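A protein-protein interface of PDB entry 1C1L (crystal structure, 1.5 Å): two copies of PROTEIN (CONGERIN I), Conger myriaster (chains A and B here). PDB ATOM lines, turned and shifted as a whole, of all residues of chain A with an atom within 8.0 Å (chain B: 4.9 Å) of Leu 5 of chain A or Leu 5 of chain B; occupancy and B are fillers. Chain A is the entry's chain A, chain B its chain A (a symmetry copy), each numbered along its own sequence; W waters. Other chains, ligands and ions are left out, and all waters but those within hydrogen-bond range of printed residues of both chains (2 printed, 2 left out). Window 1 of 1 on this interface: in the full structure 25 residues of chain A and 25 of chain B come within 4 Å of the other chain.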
ATOM      1  N   GLY A   3     -15.914   3.062 -31.809  1.00  0.00           N
ATOM      2  CA  GLY A   3     -17.193   2.575 -31.358  1.00  0.00           C
ATOM      3  C   GLY A   3     -16.963   2.256 -29.903  1.00  0.00           C
ATOM      4  O   GLY A   3     -15.934   1.649 -29.611  1.00  0.00           O
ATOM      5  N   GLY A   4     -17.877   2.689 -29.063  1.00  0.00           N
ATOM      6  CA  GLY A   4     -17.691   2.593 -27.646  1.00  0.00           C
ATOM      7  C   GLY A   4     -17.360   4.002 -27.196  1.00  0.00           C
ATOM      8  O   GLY A   4     -17.194   4.929 -28.013  1.00  0.00           O
ATOM      9  N   LEU A   5     -17.295   4.084 -25.891  1.00  0.00           N
ATOM     10  CA  LEU A   5     -17.011   5.323 -25.211  1.00  0.00           C
ATOM     11  C   LEU A   5     -15.910   5.035 -24.218  1.00  0.00           C
ATOM     12  O   LEU A   5     -15.979   4.086 -23.429  1.00  0.00           O
ATOM     13  CB  LEU A   5     -18.237   5.809 -24.465  1.00  0.00           C
ATOM     14  CG  LEU A   5     -18.120   7.129 -23.730  1.00  0.00           C
ATOM     15  CD1 LEU A   5     -17.949   8.270 -24.725  1.00  0.00           C
ATOM     16  CD2 LEU A   5     -19.343   7.278 -22.841  1.00  0.00           C
ATOM     17  N   GLN A   6     -14.856   5.843 -24.277  1.00  0.00           N
ATOM     18  CA  GLN A   6     -13.770   5.803 -23.334  1.00  0.00           C
ATOM     19  C   GLN A   6     -14.152   6.731 -22.187  1.00  0.00           C
ATOM     20  O   GLN A   6     -14.293   7.944 -22.401  1.00  0.00           O
ATOM     21  CB  GLN A   6     -12.492   6.280 -24.018  1.00  0.00           C
ATOM     22  CG  GLN A   6     -11.294   6.291 -23.070  1.00  0.00           C
ATOM     23  CD  GLN A   6     -10.913   4.930 -22.509  1.00  0.00           C
ATOM     24  OE1 GLN A   6     -10.406   4.804 -21.404  1.00  0.00           O
ATOM     25  NE2 GLN A   6     -11.122   3.840 -23.222  1.00  0.00           N
ATOM     26  N   VAL A   7     -14.354   6.195 -20.989  1.00  0.00           N
ATOM     27  CA  VAL A   7     -14.671   6.980 -19.811  1.00  0.00           C
ATOM     28  C   VAL A   7     -13.371   7.045 -19.015  1.00  0.00           C
ATOM     29  O   VAL A   7     -13.017   6.136 -18.259  1.00  0.00           O
ATOM     30  CB  VAL A   7     -15.805   6.284 -19.012  1.00  0.00           C
ATOM     31  CG1 VAL A   7     -16.159   7.154 -17.821  1.00  0.00           C
ATOM     32  CG2 VAL A   7     -17.019   6.033 -19.893  1.00  0.00           C
ATOM     33  N   LYS A   8     -12.675   8.178 -19.166  1.00  0.00           N
ATOM     34  CA  LYS A   8     -11.351   8.379 -18.598  1.00  0.00           C
ATOM     35  C   LYS A   8     -11.256   8.157 -17.096  1.00  0.00           C
ATOM     36  O   LYS A   8     -10.298   7.579 -16.581  1.00  0.00           O
ATOM     37  CB  LYS A   8     -10.850   9.801 -18.880  1.00  0.00           C
ATOM     38  CG  LYS A   8      -9.402   9.982 -18.420  1.00  0.00           C
ATOM     39  CD  LYS A   8      -8.988  11.439 -18.350  1.00  0.00           C
ATOM     40  CE  LYS A   8      -8.085  11.681 -17.148  1.00  0.00           C
ATOM     41  NZ  LYS A   8      -8.779  11.363 -15.910  1.00  0.00           N
ATOM     42  N   ASN A   9     -12.305   8.558 -16.393  1.00  0.00           N
ATOM     43  CA  ASN A   9     -12.319   8.523 -14.938  1.00  0.00           C
ATOM     44  C   ASN A   9     -12.509   7.176 -14.294  1.00  0.00           C
ATOM     45  O   ASN A   9     -12.281   7.036 -13.097  1.00  0.00           O
ATOM     46  CB  ASN A   9     -13.408   9.419 -14.384  1.00  0.00           C
ATOM     47  CG  ASN A   9     -13.220  10.843 -14.849  1.00  0.00           C
ATOM     48  OD1 ASN A   9     -13.449  11.143 -16.017  1.00  0.00           O
ATOM     49  ND2 ASN A   9     -12.780  11.728 -13.972  1.00  0.00           N
ATOM     50  N   PHE A  10     -12.980   6.207 -15.067  1.00  0.00           N
ATOM     51  CA  PHE A  10     -13.318   4.923 -14.491  1.00  0.00           C
ATOM     52  C   PHE A  10     -12.178   3.920 -14.576  1.00  0.00           C
ATOM     53  O   PHE A  10     -11.926   3.353 -15.635  1.00  0.00           O
ATOM     54  CB  PHE A  10     -14.571   4.354 -15.189  1.00  0.00           C
ATOM     55  CG  PHE A  10     -15.926   4.939 -14.786  1.00  0.00           C
ATOM     56  CD1 PHE A  10     -16.052   5.927 -13.797  1.00  0.00           C
ATOM     57  CD2 PHE A  10     -17.078   4.453 -15.405  1.00  0.00           C
ATOM     58  CE1 PHE A  10     -17.308   6.410 -13.446  1.00  0.00           C
ATOM     59  CE2 PHE A  10     -18.331   4.941 -15.042  1.00  0.00           C
ATOM     60  CZ  PHE A  10     -18.445   5.915 -14.064  1.00  0.00           C
ATOM     61  N   ASP A  11     -11.418   3.741 -13.506  1.00  0.00           N
ATOM     62  CA  ASP A  11     -10.375   2.731 -13.469  1.00  0.00           C
ATOM     63  C   ASP A  11     -10.926   1.595 -12.651  1.00  0.00           C
ATOM     64  O   ASP A  11     -11.010   1.662 -11.421  1.00  0.00           O
ATOM     65  CB  ASP A  11      -9.104   3.204 -12.783  1.00  0.00           C
ATOM     66  CG  ASP A  11      -8.370   4.321 -13.479  1.00  0.00           C
ATOM     67  OD1 ASP A  11      -8.355   4.354 -14.700  1.00  0.00           O
ATOM     68  OD2 ASP A  11      -7.808   5.166 -12.792  1.00  0.00           O
ATOM     69  N   PHE A  12     -11.339   0.531 -13.312  1.00  0.00           N
ATOM     70  CA  PHE A  12     -11.885  -0.608 -12.609  1.00  0.00           C
ATOM     71  C   PHE A  12     -10.703  -1.436 -12.129  1.00  0.00           C
ATOM     72  O   PHE A  12     -10.184  -2.307 -12.833  1.00  0.00           O
ATOM     73  CB  PHE A  12     -12.804  -1.390 -13.571  1.00  0.00           C
ATOM     74  CG  PHE A  12     -13.529  -2.557 -12.911  1.00  0.00           C
ATOM     75  CD1 PHE A  12     -13.871  -2.503 -11.561  1.00  0.00           C
ATOM     76  CD2 PHE A  12     -13.839  -3.693 -13.659  1.00  0.00           C
ATOM     77  CE1 PHE A  12     -14.518  -3.572 -10.948  1.00  0.00           C
ATOM     78  CE2 PHE A  12     -14.490  -4.764 -13.043  1.00  0.00           C
ATOM     79  CZ  PHE A  12     -14.830  -4.706 -11.691  1.00  0.00           C
ATOM     80  N   LEU A  18     -18.000  -2.038  -9.924  1.00  0.00           N
ATOM     81  CA  LEU A  18     -18.549  -1.668 -11.210  1.00  0.00           C
ATOM     82  C   LEU A  18     -19.981  -2.188 -11.307  1.00  0.00           C
ATOM     83  O   LEU A  18     -20.207  -3.394 -11.168  1.00  0.00           O
ATOM     84  CB  LEU A  18     -17.707  -2.273 -12.327  1.00  0.00           C
ATOM     85  CG  LEU A  18     -18.181  -2.076 -13.757  1.00  0.00           C
ATOM     86  CD1 LEU A  18     -17.997  -0.619 -14.134  1.00  0.00           C
ATOM     87  CD2 LEU A  18     -17.388  -2.953 -14.706  1.00  0.00           C
ATOM     88  N   THR A  19     -20.988  -1.349 -11.470  1.00  0.00           N
ATOM     89  CA  THR A  19     -22.356  -1.808 -11.646  1.00  0.00           C
ATOM     90  C   THR A  19     -22.732  -1.596 -13.098  1.00  0.00           C
ATOM     91  O   THR A  19     -22.462  -0.526 -13.647  1.00  0.00           O
ATOM     92  CB  THR A  19     -23.317  -1.019 -10.742  1.00  0.00           C
ATOM     93  OG1 THR A  19     -22.922  -1.330  -9.413  1.00  0.00           O
ATOM     94  CG2 THR A  19     -24.793  -1.363 -10.920  1.00  0.00           C
ATOM     95  N   VAL A  20     -23.308  -2.611 -13.735  1.00  0.00           N
ATOM     96  CA  VAL A  20     -23.844  -2.465 -15.066  1.00  0.00           C
ATOM     97  C   VAL A  20     -25.357  -2.598 -14.911  1.00  0.00           C
ATOM     98  O   VAL A  20     -25.853  -3.406 -14.106  1.00  0.00           O
ATOM     99  CB  VAL A  20     -23.281  -3.561 -16.019  1.00  0.00           C
ATOM    100  CG1 VAL A  20     -21.805  -3.276 -16.257  1.00  0.00           C
ATOM    101  CG2 VAL A  20     -23.429  -4.959 -15.433  1.00  0.00           C
ATOM    102  N   ASN A  34     -19.291  -8.922 -20.211  1.00  0.00           N
ATOM    103  CA  ASN A  34     -17.923  -9.307 -20.495  1.00  0.00           C
ATOM    104  C   ASN A  34     -16.945  -8.246 -20.017  1.00  0.00           C
ATOM    105  O   ASN A  34     -17.090  -7.090 -20.412  1.00  0.00           O
ATOM    106  CB  ASN A  34     -17.724  -9.470 -21.995  1.00  0.00           C
ATOM    107  CG  ASN A  34     -18.753 -10.413 -22.579  1.00  0.00           C
ATOM    108  OD1 ASN A  34     -18.615 -11.636 -22.518  1.00  0.00           O
ATOM    109  ND2 ASN A  34     -19.857  -9.891 -23.101  1.00  0.00           N
ATOM    110  N   VAL A  35     -15.991  -8.592 -19.149  1.00  0.00           N
ATOM    111  CA  VAL A  35     -14.930  -7.666 -18.750  1.00  0.00           C
ATOM    112  C   VAL A  35     -13.574  -8.311 -18.985  1.00  0.00           C
ATOM    113  O   VAL A  35     -13.355  -9.524 -18.784  1.00  0.00           O
ATOM    114  CB  VAL A  35     -14.970  -7.234 -17.239  1.00  0.00           C
ATOM    115  CG1 VAL A  35     -16.134  -6.286 -17.048  1.00  0.00           C
ATOM    116  CG2 VAL A  35     -15.100  -8.421 -16.297  1.00  0.00           C
ATOM    117  N   GLY A  36     -12.641  -7.494 -19.444  1.00  0.00           N
ATOM    118  CA  GLY A  36     -11.312  -7.979 -19.697  1.00  0.00           C
ATOM    119  C   GLY A  36     -10.499  -6.914 -20.386  1.00  0.00           C
ATOM    120  O   GLY A  36     -10.655  -5.717 -20.122  1.00  0.00           O
ATOM    121  N   PHE A 119      -6.340  -4.713 -13.057  1.00  0.00           N
ATOM    122  CA  PHE A 119      -6.954  -3.600 -13.756  1.00  0.00           C
ATOM    123  C   PHE A 119      -7.644  -4.205 -14.981  1.00  0.00           C
ATOM    124  O   PHE A 119      -7.053  -5.085 -15.631  1.00  0.00           O
ATOM    125  CB  PHE A 119      -5.876  -2.587 -14.186  1.00  0.00           C
ATOM    126  CG  PHE A 119      -6.452  -1.486 -15.061  1.00  0.00           C
ATOM    127  CD1 PHE A 119      -7.399  -0.605 -14.535  1.00  0.00           C
ATOM    128  CD2 PHE A 119      -6.093  -1.411 -16.408  1.00  0.00           C
ATOM    129  CE1 PHE A 119      -7.992   0.336 -15.364  1.00  0.00           C
ATOM    130  CE2 PHE A 119      -6.694  -0.464 -17.231  1.00  0.00           C
ATOM    131  CZ  PHE A 119      -7.643   0.408 -16.709  1.00  0.00           C
ATOM    132  N   LEU A 120      -8.872  -3.792 -15.304  1.00  0.00           N
ATOM    133  CA  LEU A 120      -9.595  -4.308 -16.464  1.00  0.00           C
ATOM    134  C   LEU A 120     -10.087  -3.139 -17.312  1.00  0.00           C
ATOM    135  O   LEU A 120     -10.968  -2.398 -16.861  1.00  0.00           O
ATOM    136  CB  LEU A 120     -10.808  -5.131 -16.057  1.00  0.00           C
ATOM    137  CG  LEU A 120     -10.526  -6.404 -15.273  1.00  0.00           C
ATOM    138  CD1 LEU A 120     -11.830  -6.979 -14.775  1.00  0.00           C
ATOM    139  CD2 LEU A 120      -9.837  -7.426 -16.156  1.00  0.00           C
ATOM    140  N   PRO A 121      -9.538  -2.897 -18.503  1.00  0.00           N
ATOM    141  CA  PRO A 121      -9.848  -1.736 -19.344  1.00  0.00           C
ATOM    142  C   PRO A 121     -11.086  -1.817 -20.220  1.00  0.00           C
ATOM    143  O   PRO A 121     -11.487  -0.817 -20.817  1.00  0.00           O
ATOM    144  CB  PRO A 121      -8.595  -1.556 -20.152  1.00  0.00           C
ATOM    145  CG  PRO A 121      -8.213  -2.988 -20.430  1.00  0.00           C
ATOM    146  CD  PRO A 121      -8.402  -3.625 -19.067  1.00  0.00           C
ATOM    147  N   PHE A 122     -11.692  -2.993 -20.351  1.00  0.00           N
ATOM    148  CA  PHE A 122     -12.754  -3.185 -21.315  1.00  0.00           C
ATOM    149  C   PHE A 122     -14.011  -3.826 -20.736  1.00  0.00           C
ATOM    150  O   PHE A 122     -13.947  -4.779 -19.947  1.00  0.00           O
ATOM    151  CB  PHE A 122     -12.171  -4.031 -22.448  1.00  0.00           C
ATOM    152  CG  PHE A 122     -13.150  -4.436 -23.534  1.00  0.00           C
ATOM    153  CD1 PHE A 122     -13.339  -3.600 -24.631  1.00  0.00           C
ATOM    154  CD2 PHE A 122     -13.865  -5.635 -23.422  1.00  0.00           C
ATOM    155  CE1 PHE A 122     -14.249  -3.965 -25.627  1.00  0.00           C
ATOM    156  CE2 PHE A 122     -14.774  -5.990 -24.417  1.00  0.00           C
ATOM    157  CZ  PHE A 122     -14.962  -5.155 -25.515  1.00  0.00           C
ATOM    158  N   LEU A 123     -15.137  -3.296 -21.204  1.00  0.00           N
ATOM    159  CA  LEU A 123     -16.448  -3.796 -20.822  1.00  0.00           C
ATOM    160  C   LEU A 123     -17.360  -3.875 -22.038  1.00  0.00           C
ATOM    161  O   LEU A 123     -17.421  -2.932 -22.842  1.00  0.00           O
ATOM    162  CB  LEU A 123     -17.090  -2.863 -19.777  1.00  0.00           C
ATOM    163  CG  LEU A 123     -18.590  -3.044 -19.428  1.00  0.00           C
ATOM    164  CD1 LEU A 123     -18.797  -4.344 -18.685  1.00  0.00           C
ATOM    165  CD2 LEU A 123     -19.075  -1.874 -18.603  1.00  0.00           C
ATOM    166  N   SER A 124     -18.079  -4.994 -22.193  1.00  0.00           N
ATOM    167  CA  SER A 124     -19.113  -5.081 -23.201  1.00  0.00           C
ATOM    168  C   SER A 124     -20.276  -5.907 -22.673  1.00  0.00           C
ATOM    169  O   SER A 124     -20.120  -6.792 -21.820  1.00  0.00           O
ATOM    170  CB  SER A 124     -18.567  -5.736 -24.495  1.00  0.00           C
ATOM    171  OG  SER A 124     -18.199  -7.116 -24.438  1.00  0.00           O
ATOM    172  N   VAL A 134     -23.575   2.480 -16.508  1.00  0.00           N
ATOM    173  CA  VAL A 134     -22.343   1.990 -15.930  1.00  0.00           C
ATOM    174  C   VAL A 134     -22.038   2.929 -14.780  1.00  0.00           C
ATOM    175  O   VAL A 134     -22.011   4.162 -14.914  1.00  0.00           O
ATOM    176  CB  VAL A 134     -21.153   2.021 -16.917  1.00  0.00           C
ATOM    177  CG1 VAL A 134     -19.876   1.583 -16.207  1.00  0.00           C
ATOM    178  CG2 VAL A 134     -21.396   1.068 -18.059  1.00  0.00           C
ATOM    179  N   LYS A 135     -21.798   2.310 -13.644  1.00  0.00           N
ATOM    180  CA  LYS A 135     -21.509   3.033 -12.435  1.00  0.00           C
ATOM    181  C   LYS A 135     -20.240   2.467 -11.823  1.00  0.00           C
ATOM    182  O   LYS A 135     -19.996   1.258 -11.919  1.00  0.00           O
ATOM    183  CB  LYS A 135     -22.734   2.862 -11.591  1.00  0.00           C
ATOM    184  CG  LYS A 135     -22.682   3.355 -10.172  1.00  0.00           C
ATOM    185  CD  LYS A 135     -24.114   3.348  -9.714  1.00  0.00           C
ATOM    186  CE  LYS A 135     -24.201   3.653  -8.245  1.00  0.00           C
ATOM    187  NZ  LYS A 135     -23.676   4.971  -7.928  1.00  0.00           N
ATOM    188  N   LEU A 136     -19.393   3.297 -11.221  1.00  0.00           N
ATOM    189  CA  LEU A 136     -18.194   2.817 -10.577  1.00  0.00           C
ATOM    190  C   LEU A 136     -18.076   3.555  -9.258  1.00  0.00           C
ATOM    191  O   LEU A 136     -18.244   4.775  -9.216  1.00  0.00           O
ATOM    192  CB  LEU A 136     -16.975   3.089 -11.452  1.00  0.00           C
ATOM    193  CG  LEU A 136     -15.664   2.528 -10.928  1.00  0.00           C
ATOM    194  CD1 LEU A 136     -15.650   1.033 -11.153  1.00  0.00           C
ATOM    195  CD2 LEU A 136     -14.494   3.162 -11.633  1.00  0.00           C
ATOM    196  N   GLY B   3      -5.939   3.432 -18.449  1.00  0.00           N
ATOM    197  CA  GLY B   3      -6.647   4.152 -17.422  1.00  0.00           C
ATOM    198  C   GLY B   3      -7.916   4.594 -18.104  1.00  0.00           C
ATOM    199  O   GLY B   3      -7.818   5.068 -19.236  1.00  0.00           O
ATOM    200  N   GLY B   4      -9.032   4.400 -17.437  1.00  0.00           N
ATOM    201  CA  GLY B   4     -10.310   4.624 -18.040  1.00  0.00           C
ATOM    202  C   GLY B   4     -10.859   3.241 -18.329  1.00  0.00           C
ATOM    203  O   GLY B   4     -10.176   2.214 -18.143  1.00  0.00           O
ATOM    204  N   LEU B   5     -12.091   3.296 -18.767  1.00  0.00           N
ATOM    205  CA  LEU B   5     -12.844   2.113 -19.098  1.00  0.00           C
ATOM    206  C   LEU B   5     -13.439   2.341 -20.468  1.00  0.00           C
ATOM    207  O   LEU B   5     -14.064   3.372 -20.740  1.00  0.00           O
ATOM    208  CB  LEU B   5     -13.964   1.903 -18.100  1.00  0.00           C
ATOM    209  CG  LEU B   5     -14.829   0.672 -18.279  1.00  0.00           C
ATOM    210  CD1 LEU B   5     -14.008  -0.586 -18.021  1.00  0.00           C
ATOM    211  CD2 LEU B   5     -16.033   0.808 -17.363  1.00  0.00           C
ATOM    212  N   GLN B   6     -13.213   1.383 -21.360  1.00  0.00           N
ATOM    213  CA  GLN B   6     -13.801   1.364 -22.672  1.00  0.00           C
ATOM    214  C   GLN B   6     -15.135   0.638 -22.544  1.00  0.00           C
ATOM    215  O   GLN B   6     -15.154  -0.557 -22.212  1.00  0.00           O
ATOM    216  CB  GLN B   6     -12.870   0.627 -23.631  1.00  0.00           C
ATOM    217  CG  GLN B   6     -13.440   0.542 -25.046  1.00  0.00           C
ATOM    218  CD  GLN B   6     -13.663   1.884 -25.725  1.00  0.00           C
ATOM    219  OE1 GLN B   6     -14.552   2.055 -26.546  1.00  0.00           O
ATOM    220  NE2 GLN B   6     -12.880   2.907 -25.438  1.00  0.00           N
ATOM    221  N   VAL B   7     -16.248   1.329 -22.765  1.00  0.00           N
ATOM    222  CA  VAL B   7     -17.571   0.737 -22.723  1.00  0.00           C
ATOM    223  C   VAL B   7     -17.977   0.567 -24.184  1.00  0.00           C
ATOM    224  O   VAL B   7     -18.460   1.491 -24.844  1.00  0.00           O
ATOM    225  CB  VAL B   7     -18.539   1.681 -21.960  1.00  0.00           C
ATOM    226  CG1 VAL B   7     -19.898   1.012 -21.877  1.00  0.00           C
ATOM    227  CG2 VAL B   7     -18.001   2.011 -20.577  1.00  0.00           C
ATOM    228  N   PHE B  10     -21.490   1.772 -25.811  1.00  0.00           N
ATOM    229  CA  PHE B  10     -21.937   3.149 -25.804  1.00  0.00           C
ATOM    230  C   PHE B  10     -21.390   3.953 -26.973  1.00  0.00           C
ATOM    231  O   PHE B  10     -20.230   4.353 -26.963  1.00  0.00           O
ATOM    232  CB  PHE B  10     -21.535   3.818 -24.472  1.00  0.00           C
ATOM    233  CG  PHE B  10     -22.381   3.492 -23.240  1.00  0.00           C
ATOM    234  CD1 PHE B  10     -23.503   2.651 -23.300  1.00  0.00           C
ATOM    235  CD2 PHE B  10     -22.039   4.073 -22.018  1.00  0.00           C
ATOM    236  CE1 PHE B  10     -24.256   2.405 -22.157  1.00  0.00           C
ATOM    237  CE2 PHE B  10     -22.804   3.824 -20.881  1.00  0.00           C
ATOM    238  CZ  PHE B  10     -23.910   2.993 -20.952  1.00  0.00           C
ATOM    239  N   PHE B  12     -21.848   7.298 -28.519  1.00  0.00           N
ATOM    240  CA  PHE B  12     -22.495   8.577 -28.336  1.00  0.00           C
ATOM    241  C   PHE B  12     -22.499   9.266 -29.692  1.00  0.00           C
ATOM    242  O   PHE B  12     -21.557   9.965 -30.074  1.00  0.00           O
ATOM    243  CB  PHE B  12     -21.718   9.376 -27.267  1.00  0.00           C
ATOM    244  CG  PHE B  12     -22.370  10.705 -26.904  1.00  0.00           C
ATOM    245  CD1 PHE B  12     -23.755  10.854 -26.971  1.00  0.00           C
ATOM    246  CD2 PHE B  12     -21.575  11.784 -26.517  1.00  0.00           C
ATOM    247  CE1 PHE B  12     -24.354  12.070 -26.657  1.00  0.00           C
ATOM    248  CE2 PHE B  12     -22.179  13.003 -26.200  1.00  0.00           C
ATOM    249  CZ  PHE B  12     -23.565  13.148 -26.269  1.00  0.00           C
ATOM    250  N   LEU B  18     -26.520  11.201 -23.482  1.00  0.00           N
ATOM    251  CA  LEU B  18     -25.507  10.776 -22.541  1.00  0.00           C
ATOM    252  C   LEU B  18     -25.734  11.491 -21.212  1.00  0.00           C
ATOM    253  O   LEU B  18     -25.746  12.726 -21.173  1.00  0.00           O
ATOM    254  CB  LEU B  18     -24.123  11.119 -23.079  1.00  0.00           C
ATOM    255  CG  LEU B  18     -22.927  10.837 -22.186  1.00  0.00           C
ATOM    256  CD1 LEU B  18     -22.737   9.336 -22.087  1.00  0.00           C
ATOM    257  CD2 LEU B  18     -21.674  11.473 -22.757  1.00  0.00           C
ATOM    258  N   LEU B 120     -18.625  10.950 -30.759  1.00  0.00           N
ATOM    259  CA  LEU B 120     -17.646  11.436 -29.788  1.00  0.00           C
ATOM    260  C   LEU B 120     -17.154  10.267 -28.940  1.00  0.00           C
ATOM    261  O   LEU B 120     -17.937   9.722 -28.155  1.00  0.00           O
ATOM    262  CB  LEU B 120     -18.244  12.473 -28.849  1.00  0.00           C
ATOM    263  CG  LEU B 120     -18.719  13.768 -29.490  1.00  0.00           C
ATOM    264  CD1 LEU B 120     -19.466  14.585 -28.462  1.00  0.00           C
ATOM    265  CD2 LEU B 120     -17.537  14.570 -29.998  1.00  0.00           C
ATOM    266  N   PRO B 121     -15.907   9.813 -29.084  1.00  0.00           N
ATOM    267  CA  PRO B 121     -15.370   8.626 -28.412  1.00  0.00           C
ATOM    268  C   PRO B 121     -14.868   8.793 -26.988  1.00  0.00           C
ATOM    269  O   PRO B 121     -14.563   7.804 -26.321  1.00  0.00           O
ATOM    270  CB  PRO B 121     -14.283   8.170 -29.344  1.00  0.00           C
ATOM    271  CG  PRO B 121     -13.698   9.488 -29.785  1.00  0.00           C
ATOM    272  CD  PRO B 121     -14.948  10.295 -30.078  1.00  0.00           C
ATOM    273  N   PHE B 122     -14.735  10.025 -26.506  1.00  0.00           N
ATOM    274  CA  PHE B 122     -14.085  10.266 -25.236  1.00  0.00           C
ATOM    275  C   PHE B 122     -14.886  11.148 -24.285  1.00  0.00           C
ATOM    276  O   PHE B 122     -15.474  12.163 -24.685  1.00  0.00           O
ATOM    277  CB  PHE B 122     -12.721  10.882 -25.551  1.00  0.00           C
ATOM    278  CG  PHE B 122     -11.901  11.306 -24.347  1.00  0.00           C
ATOM    279  CD1 PHE B 122     -11.037  10.391 -23.751  1.00  0.00           C
ATOM    280  CD2 PHE B 122     -12.024  12.604 -23.835  1.00  0.00           C
ATOM    281  CE1 PHE B 122     -10.289  10.775 -22.635  1.00  0.00           C
ATOM    282  CE2 PHE B 122     -11.278  12.978 -22.719  1.00  0.00           C
ATOM    283  CZ  PHE B 122     -10.413  12.063 -22.125  1.00  0.00           C
ATOM    284  N   LEU B 123     -14.833  10.745 -23.019  1.00  0.00           N
ATOM    285  CA  LEU B 123     -15.483  11.476 -21.943  1.00  0.00           C
ATOM    286  C   LEU B 123     -14.569  11.555 -20.729  1.00  0.00           C
ATOM    287  O   LEU B 123     -13.965  10.548 -20.328  1.00  0.00           O
ATOM    288  CB  LEU B 123     -16.792  10.773 -21.538  1.00  0.00           C
ATOM    289  CG  LEU B 123     -17.512  11.216 -20.237  1.00  0.00           C
ATOM    290  CD1 LEU B 123     -18.079  12.606 -20.404  1.00  0.00           C
ATOM    291  CD2 LEU B 123     -18.605  10.231 -19.888  1.00  0.00           C
ATOM    292  N   VAL B 134     -22.493   6.865 -15.747  1.00  0.00           N
ATOM    293  CA  VAL B 134     -22.627   7.226 -17.142  1.00  0.00           C
ATOM    294  C   VAL B 134     -23.775   6.387 -17.664  1.00  0.00           C
ATOM    295  O   VAL B 134     -23.826   5.156 -17.513  1.00  0.00           O
ATOM    296  CB  VAL B 134     -21.366   6.906 -17.977  1.00  0.00           C
ATOM    297  CG1 VAL B 134     -21.620   7.224 -19.448  1.00  0.00           C
ATOM    298  CG2 VAL B 134     -20.206   7.751 -17.517  1.00  0.00           C
HETATM  299  O   HOH W   1     -13.757   5.140 -27.534  1.00  0.00           O
HETATM  300  O   HOH W   2      -9.711   1.544 -21.523  1.00  0.00           O
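O of Gly 3 of chain A lies close to OE1 of Gln 6 of chain B (3.4 Å). The backbone NH (N) of Leu 5 of chain A is in hydrogen-bond range of the side-chain amide oxygen (OE1) of Gln 6 of chain B (3.5 Å). The backbone carbonyl oxygen (O) of Leu 5 of chain A is in hydrogen-bond range of the backbone NH (N) of Val 7 of chain B, 2.8 Å away. N of Leu 5 of chain A is in hydrogen-bond range of O of Phe 10 of chain B, 3.1 Å away. O of Gly 3 of chain B sits close to OE1 of Gln 6 of chain A (3.4 Å). N of Leu 5 of chain B sits at hydrogen-bond distance from OE1 of Gln 6 of chain A. The side-chain amide nitrogen (NE2) of Gln 6 of chain A sits close to the side-chain amide nitrogen (NE2) of Gln 6 of chain B (3.0 Å). The backbone NH (N) of Gln 6 of chain A lies within hydrogen-bond range of the backbone carbonyl oxygen (O) of Pro 121 of chain B. The backbone carbonyl oxygen of Gln 6 of chain A sits at hydrogen-bond distance from the backbone NH of Leu 123 of chain B (2.9 Å). N of Val 7 of chain A is in hydrogen-bond range of O of Leu 5 of chain B (2.8 Å). N of Lys 8 of chain A sits at hydrogen-bond distance from O of Leu 123 of chain B. The backbone NH (N) of Leu 5 of chain B sits at hydrogen-bond distance from the backbone carbonyl oxygen (O) of Phe 10 of chain A, at 3.1 Å. N of Gly 4 of chain B is in hydrogen-bond range of OD1 of Asp 11 of chain A (2.8 Å). N of Gln 6 of chain B is in hydrogen-bond range of O of Pro 121 of chain A, 2.8 Å away. O of Gln 6 of chain B is in hydrogen-bond range of N of Leu 123 of chain A, at 2.9 Å. N of Val 134 of chain A lies within hydrogen-bond range of O of Val 134 of chain B (2.9 Å). O of Gly 4 of chain A lies close to O of Phe 10 of chain B. The backbone carbonyl oxygen (O) of Leu 5 of chain A sits close to the backbone carbonyl oxygen (O) of Leu 5 of chain B (3.4 Å). The backbone carbonyl oxygen (O) of Gly 4 of chain B lies close to the backbone carbonyl oxygen (O) of Phe 10 of chain A, at 3.3 Å.
The backbone carbonyl oxygen of Phe 12 of chain B lies within hydrogen-bond range of the backbone NH of Leu 120 of chain B, at 3.2 Å.
Gly 4 of chain A touches Gln 6 of chain B. Val 7 of chain B touches Gly 4 of chain A (O to CA, 3.1 Å). Leu 5 of chain A touches Leu 120 of chain B (CD1 to O, 3.7 Å). Val 7 of chain A touches Leu 123 of chain B. Phe 122 of chain A touches Gln 6 of chain B.
Leu 5 of chain A touches just these residues of chain B: Leu 5, Gln 6, Val 7, Phe 10, Leu 120 and Pro 121. Gly 4 of chain B touches just these residues of chain A: Gln 6, Val 7, Lys 8, Phe 10, Asp 11 and Phe 119. Printed residues of chain B within 4 Å of Pro 121 of chain A: Leu 5 (3.7 Å) and Gln 6 (2.8 Å). Of the printed residues of chain A, Pro 121 of chain B touches Leu 5 (3.7 Å) and Gln 6 (2.8 Å). Phe 12 of chain A touches none of the printed residues of chain B. The nearest residue of chain A that does not touch Leu 5 of chain B is Leu 18 of chain A (4.04 Å). The nearest printed residue of chain B that does not touch Val 134 of chain A is Leu 5 of chain B (4.1 Å).
Of the 25 printed residues of chain A, 14 touch a printed residue of chain B. Hydrophobic or aromatic side chains of chain B that line the printed part of chain A: Leu 5, Val 7, Phe 10, Phe 122 and Leu 123. Among the printed residues, no Asp or Glu carboxylate lies within 4 Å of a Lys or Arg side-chain nitrogen of the other chain.
Leu 5 of chain A touches its own counterpart, Leu 5 of chain B. Val 7 of chain A touches Leu 123 of chain B, and with the chains exchanged Leu 123 of chain A touches Val 7 of chain B.
Water W2 lies within hydrogen-bond range of O of Pro 121 of chain A (3.0 Å), NE2 of Gln 6 of chain A (3.2 Å) and O of Gly 4 of chain B (3.5 Å).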
